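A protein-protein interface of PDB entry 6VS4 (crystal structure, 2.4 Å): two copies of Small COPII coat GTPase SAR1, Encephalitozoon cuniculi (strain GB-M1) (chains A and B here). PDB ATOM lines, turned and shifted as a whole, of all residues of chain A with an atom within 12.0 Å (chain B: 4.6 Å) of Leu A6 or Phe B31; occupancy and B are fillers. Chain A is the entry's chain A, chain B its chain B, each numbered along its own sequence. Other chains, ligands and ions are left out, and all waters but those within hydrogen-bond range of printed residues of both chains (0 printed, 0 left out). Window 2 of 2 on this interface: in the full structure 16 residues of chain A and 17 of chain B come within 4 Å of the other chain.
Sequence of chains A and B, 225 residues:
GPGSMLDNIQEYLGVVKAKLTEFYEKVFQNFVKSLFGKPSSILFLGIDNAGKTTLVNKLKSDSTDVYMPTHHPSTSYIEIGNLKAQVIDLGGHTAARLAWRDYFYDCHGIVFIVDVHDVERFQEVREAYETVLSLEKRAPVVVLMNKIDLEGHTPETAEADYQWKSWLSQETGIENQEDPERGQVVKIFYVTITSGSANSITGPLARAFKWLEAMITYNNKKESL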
ATOM      1  N   GLY A   3     -31.125  -6.931  -0.846  1.00  0.00           N
ATOM      2  CA  GLY A   3     -31.082  -7.353   0.543  1.00  0.00           C
ATOM      3  C   GLY A   3     -30.062  -8.447   0.802  1.00  0.00           C
ATOM      4  O   GLY A   3     -29.315  -8.404   1.782  1.00  0.00           O
ATOM      5  N   SER A   4     -30.028  -9.429  -0.103  1.00  0.00           N
ATOM      6  CA  SER A   4     -29.082 -10.536  -0.027  1.00  0.00           C
ATOM      7  C   SER A   4     -27.640 -10.091  -0.236  1.00  0.00           C
ATOM      8  O   SER A   4     -26.719 -10.869   0.040  1.00  0.00           O
ATOM      9  CB  SER A   4     -29.454 -11.612  -1.053  1.00  0.00           C
ATOM     10  OG  SER A   4     -28.766 -12.828  -0.807  1.00  0.00           O
ATOM     11  N   MET A   5     -27.425  -8.876  -0.730  1.00  0.00           N
ATOM     12  CA  MET A   5     -26.085  -8.357  -0.970  1.00  0.00           C
ATOM     13  C   MET A   5     -25.373  -7.927   0.315  1.00  0.00           C
ATOM     14  O   MET A   5     -24.138  -7.836   0.331  1.00  0.00           O
ATOM     15  CB  MET A   5     -26.201  -7.240  -2.007  1.00  0.00           C
ATOM     16  CG  MET A   5     -24.930  -6.556  -2.409  1.00  0.00           C
ATOM     17  SD  MET A   5     -25.270  -5.251  -3.604  1.00  0.00           S
ATOM     18  CE  MET A   5     -26.817  -4.619  -2.963  1.00  0.00           C
ATOM     19  N   LEU A   6     -26.117  -7.624   1.372  1.00  0.00           N
ATOM     20  CA  LEU A   6     -25.574  -7.302   2.688  1.00  0.00           C
ATOM     21  C   LEU A   6     -25.318  -8.537   3.549  1.00  0.00           C
ATOM     22  O   LEU A   6     -24.851  -8.392   4.684  1.00  0.00           O
ATOM     23  CB  LEU A   6     -26.512  -6.349   3.426  1.00  0.00           C
ATOM     24  CG  LEU A   6     -26.742  -5.025   2.701  1.00  0.00           C
ATOM     25  CD1 LEU A   6     -27.475  -4.010   3.605  1.00  0.00           C
ATOM     26  CD2 LEU A   6     -25.432  -4.463   2.153  1.00  0.00           C
ATOM     27  N   ASP A   7     -25.658  -9.731   3.064  1.00  0.00           N
ATOM     28  CA  ASP A   7     -25.559 -10.952   3.862  1.00  0.00           C
ATOM     29  C   ASP A   7     -24.139 -11.222   4.338  1.00  0.00           C
ATOM     30  O   ASP A   7     -23.216 -11.348   3.528  1.00  0.00           O
ATOM     31  CB  ASP A   7     -26.066 -12.142   3.047  1.00  0.00           C
ATOM     32  CG  ASP A   7     -27.579 -12.298   3.118  1.00  0.00           C
ATOM     33  OD1 ASP A   7     -28.167 -12.010   4.185  1.00  0.00           O
ATOM     34  OD2 ASP A   7     -28.181 -12.711   2.104  1.00  0.00           O
ATOM     35  N   ASN A   8     -23.979 -11.322   5.664  1.00  0.00           N
ATOM     36  CA  ASN A   8     -22.749 -11.695   6.357  1.00  0.00           C
ATOM     37  C   ASN A   8     -21.678 -10.620   6.324  1.00  0.00           C
ATOM     38  O   ASN A   8     -20.582 -10.854   6.836  1.00  0.00           O
ATOM     39  CB  ASN A   8     -22.147 -13.003   5.829  1.00  0.00           C
ATOM     40  CG  ASN A   8     -23.052 -14.183   6.062  1.00  0.00           C
ATOM     41  OD1 ASN A   8     -23.621 -14.335   7.141  1.00  0.00           O
ATOM     42  ND2 ASN A   8     -23.222 -15.011   5.040  1.00  0.00           N
ATOM     43  N   ILE A   9     -21.935  -9.469   5.706  1.00  0.00           N
ATOM     44  CA  ILE A   9     -20.940  -8.404   5.687  1.00  0.00           C
ATOM     45  C   ILE A   9     -20.605  -7.963   7.110  1.00  0.00           C
ATOM     46  O   ILE A   9     -19.436  -7.764   7.459  1.00  0.00           O
ATOM     47  CB  ILE A   9     -21.454  -7.223   4.847  1.00  0.00           C
ATOM     48  CG1 ILE A   9     -21.632  -7.635   3.386  1.00  0.00           C
ATOM     49  CG2 ILE A   9     -20.498  -6.050   4.938  1.00  0.00           C
ATOM     50  CD1 ILE A   9     -20.397  -8.241   2.759  1.00  0.00           C
ATOM     51  N   GLN A  10     -21.628  -7.811   7.953  1.00  0.00           N
ATOM     52  CA  GLN A  10     -21.408  -7.360   9.319  1.00  0.00           C
ATOM     53  C   GLN A  10     -20.641  -8.403  10.137  1.00  0.00           C
ATOM     54  O   GLN A  10     -19.778  -8.048  10.952  1.00  0.00           O
ATOM     55  CB  GLN A  10     -22.766  -7.017   9.928  1.00  0.00           C
ATOM     56  CG  GLN A  10     -23.081  -5.543   9.802  1.00  0.00           C
ATOM     57  CD  GLN A  10     -24.445  -5.177  10.326  1.00  0.00           C
ATOM     58  OE1 GLN A  10     -25.272  -6.052  10.589  1.00  0.00           O
ATOM     59  NE2 GLN A  10     -24.696  -3.876  10.479  1.00  0.00           N
ATOM     60  N   GLU A  11     -20.941  -9.694   9.944  1.00  0.00           N
ATOM     61  CA  GLU A  11     -20.215 -10.739  10.670  1.00  0.00           C
ATOM     62  C   GLU A  11     -18.723 -10.711  10.348  1.00  0.00           C
ATOM     63  O   GLU A  11     -17.890 -10.926  11.236  1.00  0.00           O
ATOM     64  CB  GLU A  11     -20.804 -12.112  10.357  1.00  0.00           C
ATOM     65  CG  GLU A  11     -22.124 -12.418  11.057  1.00  0.00           C
ATOM     66  CD  GLU A  11     -23.320 -11.743  10.404  1.00  0.00           C
ATOM     67  OE1 GLU A  11     -23.127 -11.001   9.418  1.00  0.00           O
ATOM     68  OE2 GLU A  11     -24.458 -11.956  10.879  1.00  0.00           O
ATOM     69  N   TYR A  12     -18.366 -10.443   9.085  1.00  0.00           N
ATOM     70  CA  TYR A  12     -16.958 -10.326   8.714  1.00  0.00           C
ATOM     71  C   TYR A  12     -16.312  -9.090   9.330  1.00  0.00           C
ATOM     72  O   TYR A  12     -15.164  -9.151   9.778  1.00  0.00           O
ATOM     73  CB  TYR A  12     -16.802 -10.299   7.190  1.00  0.00           C
ATOM     74  CG  TYR A  12     -16.647 -11.674   6.583  1.00  0.00           C
ATOM     75  CD1 TYR A  12     -15.409 -12.308   6.555  1.00  0.00           C
ATOM     76  CD2 TYR A  12     -17.741 -12.344   6.053  1.00  0.00           C
ATOM     77  CE1 TYR A  12     -15.267 -13.576   6.013  1.00  0.00           C
ATOM     78  CE2 TYR A  12     -17.611 -13.604   5.510  1.00  0.00           C
ATOM     79  CZ  TYR A  12     -16.372 -14.214   5.489  1.00  0.00           C
ATOM     80  OH  TYR A  12     -16.247 -15.467   4.947  1.00  0.00           O
ATOM     81  N   LEU A  13     -17.010  -7.952   9.336  1.00  0.00           N
ATOM     82  CA  LEU A  13     -16.460  -6.775  10.000  1.00  0.00           C
ATOM     83  C   LEU A  13     -16.195  -7.060  11.476  1.00  0.00           C
ATOM     84  O   LEU A  13     -15.167  -6.647  12.024  1.00  0.00           O
ATOM     85  CB  LEU A  13     -17.412  -5.592   9.835  1.00  0.00           C
ATOM     86  CG  LEU A  13     -17.578  -5.012   8.435  1.00  0.00           C
ATOM     87  CD1 LEU A  13     -18.737  -4.021   8.403  1.00  0.00           C
ATOM     88  CD2 LEU A  13     -16.294  -4.310   8.063  1.00  0.00           C
ATOM     89  N   GLY A  14     -17.090  -7.807  12.125  1.00  0.00           N
ATOM     90  CA  GLY A  14     -16.885  -8.129  13.527  1.00  0.00           C
ATOM     91  C   GLY A  14     -15.721  -9.072  13.756  1.00  0.00           C
ATOM     92  O   GLY A  14     -14.935  -8.883  14.690  1.00  0.00           O
ATOM     93  N   VAL B  27     -23.713  -0.284   6.802  1.00  0.00           N
ATOM     94  CA  VAL B  27     -24.517  -1.438   6.405  1.00  0.00           C
ATOM     95  C   VAL B  27     -25.923  -1.332   6.992  1.00  0.00           C
ATOM     96  O   VAL B  27     -26.917  -1.647   6.324  1.00  0.00           O
ATOM     97  CB  VAL B  27     -23.820  -2.750   6.820  1.00  0.00           C
ATOM     98  CG1 VAL B  27     -24.729  -3.939   6.562  1.00  0.00           C
ATOM     99  CG2 VAL B  27     -22.503  -2.906   6.089  1.00  0.00           C
ATOM    100  N   PHE B  28     -26.034  -0.882   8.247  1.00  0.00           N
ATOM    101  CA  PHE B  28     -27.354  -0.684   8.841  1.00  0.00           C
ATOM    102  C   PHE B  28     -28.128   0.391   8.091  1.00  0.00           C
ATOM    103  O   PHE B  28     -29.322   0.229   7.816  1.00  0.00           O
ATOM    104  CB  PHE B  28     -27.223  -0.324  10.321  1.00  0.00           C
ATOM    105  CG  PHE B  28     -28.548  -0.097  11.018  1.00  0.00           C
ATOM    106  CD1 PHE B  28     -29.350  -1.173  11.377  1.00  0.00           C
ATOM    107  CD2 PHE B  28     -28.985   1.181  11.317  1.00  0.00           C
ATOM    108  CE1 PHE B  28     -30.563  -0.980  12.012  1.00  0.00           C
ATOM    109  CE2 PHE B  28     -30.193   1.385  11.967  1.00  0.00           C
ATOM    110  CZ  PHE B  28     -30.983   0.304  12.317  1.00  0.00           C
ATOM    111  N   GLN B  29     -27.461   1.494   7.746  1.00  0.00           N
ATOM    112  CA  GLN B  29     -28.127   2.577   7.029  1.00  0.00           C
ATOM    113  C   GLN B  29     -28.620   2.123   5.663  1.00  0.00           C
ATOM    114  O   GLN B  29     -29.751   2.430   5.272  1.00  0.00           O
ATOM    115  CB  GLN B  29     -27.173   3.763   6.899  1.00  0.00           C
ATOM    116  CG  GLN B  29     -26.935   4.446   8.231  1.00  0.00           C
ATOM    117  CD  GLN B  29     -25.632   5.207   8.281  1.00  0.00           C
ATOM    118  OE1 GLN B  29     -25.174   5.751   7.277  1.00  0.00           O
ATOM    119  NE2 GLN B  29     -24.998   5.204   9.449  1.00  0.00           N
ATOM    120  N   ASN B  30     -27.788   1.374   4.927  1.00  0.00           N
ATOM    121  CA  ASN B  30     -28.195   0.878   3.615  1.00  0.00           C
ATOM    122  C   ASN B  30     -29.313  -0.147   3.733  1.00  0.00           C
ATOM    123  O   ASN B  30     -30.231  -0.172   2.902  1.00  0.00           O
ATOM    124  CB  ASN B  30     -26.998   0.304   2.867  1.00  0.00           C
ATOM    125  CG  ASN B  30     -26.198   1.379   2.165  1.00  0.00           C
ATOM    126  OD1 ASN B  30     -26.577   1.833   1.084  1.00  0.00           O
ATOM    127  ND2 ASN B  30     -25.094   1.803   2.775  1.00  0.00           N
ATOM    128  N   PHE B  31     -29.258  -0.993   4.763  1.00  0.00           N
ATOM    129  CA  PHE B  31     -30.326  -1.963   4.978  1.00  0.00           C
ATOM    130  C   PHE B  31     -31.673  -1.270   5.171  1.00  0.00           C
ATOM    131  O   PHE B  31     -32.698  -1.738   4.663  1.00  0.00           O
ATOM    132  CB  PHE B  31     -29.983  -2.843   6.177  1.00  0.00           C
ATOM    133  CG  PHE B  31     -31.170  -3.530   6.788  1.00  0.00           C
ATOM    134  CD1 PHE B  31     -31.598  -4.753   6.307  1.00  0.00           C
ATOM    135  CD2 PHE B  31     -31.832  -2.970   7.872  1.00  0.00           C
ATOM    136  CE1 PHE B  31     -32.680  -5.391   6.875  1.00  0.00           C
ATOM    137  CE2 PHE B  31     -32.917  -3.601   8.442  1.00  0.00           C
ATOM    138  CZ  PHE B  31     -33.344  -4.815   7.946  1.00  0.00           C
ATOM    139  N   VAL B  32     -31.693  -0.155   5.901  1.00  0.00           N
ATOM    140  CA  VAL B  32     -32.954   0.529   6.171  1.00  0.00           C
ATOM    141  C   VAL B  32     -33.500   1.187   4.906  1.00  0.00           C
ATOM    142  O   VAL B  32     -34.697   1.090   4.611  1.00  0.00           O
ATOM    143  CB  VAL B  32     -32.766   1.540   7.315  1.00  0.00           C
ATOM    144  CG1 VAL B  32     -33.876   2.580   7.311  1.00  0.00           C
ATOM    145  CG2 VAL B  32     -32.711   0.807   8.644  1.00  0.00           C
ATOM    146  N   LYS B  33     -32.642   1.862   4.139  1.00  0.00           N
ATOM    147  CA  LYS B  33     -33.106   2.475   2.897  1.00  0.00           C
ATOM    148  C   LYS B  33     -33.674   1.442   1.930  1.00  0.00           C
ATOM    149  O   LYS B  33     -34.615   1.741   1.181  1.00  0.00           O
ATOM    150  CB  LYS B  33     -31.973   3.251   2.222  1.00  0.00           C
ATOM    151  CG  LYS B  33     -31.616   4.551   2.909  1.00  0.00           C
ATOM    152  CD  LYS B  33     -30.840   5.476   1.991  1.00  0.00           C
ATOM    153  CE  LYS B  33     -30.534   6.794   2.687  1.00  0.00           C
ATOM    154  NZ  LYS B  33     -29.902   7.790   1.780  1.00  0.00           N
ATOM    155  N   SER B  34     -33.140   0.223   1.943  1.00  0.00           N
ATOM    156  CA  SER B  34     -33.596  -0.787   1.002  1.00  0.00           C
ATOM    157  C   SER B  34     -34.875  -1.479   1.449  1.00  0.00           C
ATOM    158  O   SER B  34     -35.466  -2.219   0.654  1.00  0.00           O
ATOM    159  CB  SER B  34     -32.490  -1.821   0.769  1.00  0.00           C
ATOM    160  OG  SER B  34     -32.449  -2.770   1.820  1.00  0.00           O
ATOM    161  N   LEU B  35     -35.324  -1.244   2.686  1.00  0.00           N
ATOM    162  CA  LEU B  35     -36.546  -1.884   3.162  1.00  0.00           C
ATOM    163  C   LEU B  35     -37.777  -1.311   2.473  1.00  0.00           C
ATOM    164  O   LEU B  35     -38.731  -2.040   2.183  1.00  0.00           O
ATOM    165  CB  LEU B  35     -36.671  -1.718   4.676  1.00  0.00           C
ATOM    166  CG  LEU B  35     -36.079  -2.820   5.556  1.00  0.00           C
ATOM    167  CD1 LEU B  35     -36.526  -2.646   7.003  1.00  0.00           C
ATOM    168  CD2 LEU B  35     -36.473  -4.185   5.026  1.00  0.00           C
ATOM    169  N   ILE B 201     -28.023  -5.863  11.489  1.00  0.00           N
ATOM    170  CA  ILE B 201     -29.199  -6.071  10.646  1.00  0.00           C
ATOM    171  C   ILE B 201     -29.897  -7.387  10.944  1.00  0.00           C
ATOM    172  O   ILE B 201     -30.863  -7.732  10.252  1.00  0.00           O
ATOM    173  CB  ILE B 201     -28.858  -5.989   9.144  1.00  0.00           C
ATOM    174  CG1 ILE B 201     -27.961  -7.146   8.721  1.00  0.00           C
ATOM    175  CG2 ILE B 201     -28.176  -4.662   8.827  1.00  0.00           C
ATOM    176  CD1 ILE B 201     -27.652  -7.116   7.259  1.00  0.00           C
ATOM    177  N   ALA B 206     -33.329  -3.936  13.981  1.00  0.00           N
ATOM    178  CA  ALA B 206     -33.505  -4.173  12.551  1.00  0.00           C
ATOM    179  C   ALA B 206     -34.676  -5.102  12.281  1.00  0.00           C
ATOM    180  O   ALA B 206     -35.346  -4.965  11.251  1.00  0.00           O
ATOM    181  CB  ALA B 206     -32.230  -4.745  11.932  1.00  0.00           C
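No position is printed for both chains.
Among the printed residues, pairs that only touch across the chains: Leu A6 with Val B27, Leu A6 with Phe B31, Ile A9 with Val B27, Gln A10 with Val B27 and Gln A10 with Phe B28.
The backbone NH of Ile B201 sits at hydrogen-bond distance from the side-chain amide oxygen of Gln A10 (2.9 Å).
The side-chain hydroxyl of Ser B34 sits at hydrogen-bond distance from the backbone carbonyl oxygen of Phe B31.
Of the 12 printed residues of chain A, 3 touch a printed residue of chain B. Hydrophobic or aromatic side chains of chain A within 4 Å of the printed part of chain B: Leu A6 and Ile A9. Hydrophobic or aromatic side chains of chain B that line the printed part of chain A: Val B27, Phe B31 and Ile B201. Among the printed residues, 6 pairs touch across the chains. Among the printed residues, no Asp or Glu carboxylate lies within 4 Å of a Lys or Arg side-chain nitrogen of the other chain.
Of the printed residues of chain B, Leu A6 touches Val B27 (3.6 Å) and Phe B31 (3.7 Å). Of the printed residues of chain B, Ile A9 touches Val B27. Of the printed residues of chain B, Gln A10 touches Val B27 (3.9 Å), Phe B28 (3.97 Å) and Ile B201 (2.9 Å). Val B27 touches just these residues of chain A: Leu A6, Ile A9 and Gln A10. No residue of chain A comes within 4 Å of Asn B30. Of the printed residues of chain A, Phe B31 touches Leu A6. No residue of chain A comes within 4 Å of Val B32. No residue of chain A comes within 4 Å of Ser B34. No residue of chain A comes within 4 Å of Leu B35. Of the printed residues of chain A, Ile B201 touches Gln A10. Ala B206 touches none of the printed residues of chain A. The nearest printed residue of chain B that does not touch Ile A9 is Ile B201 (6.4 Å).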
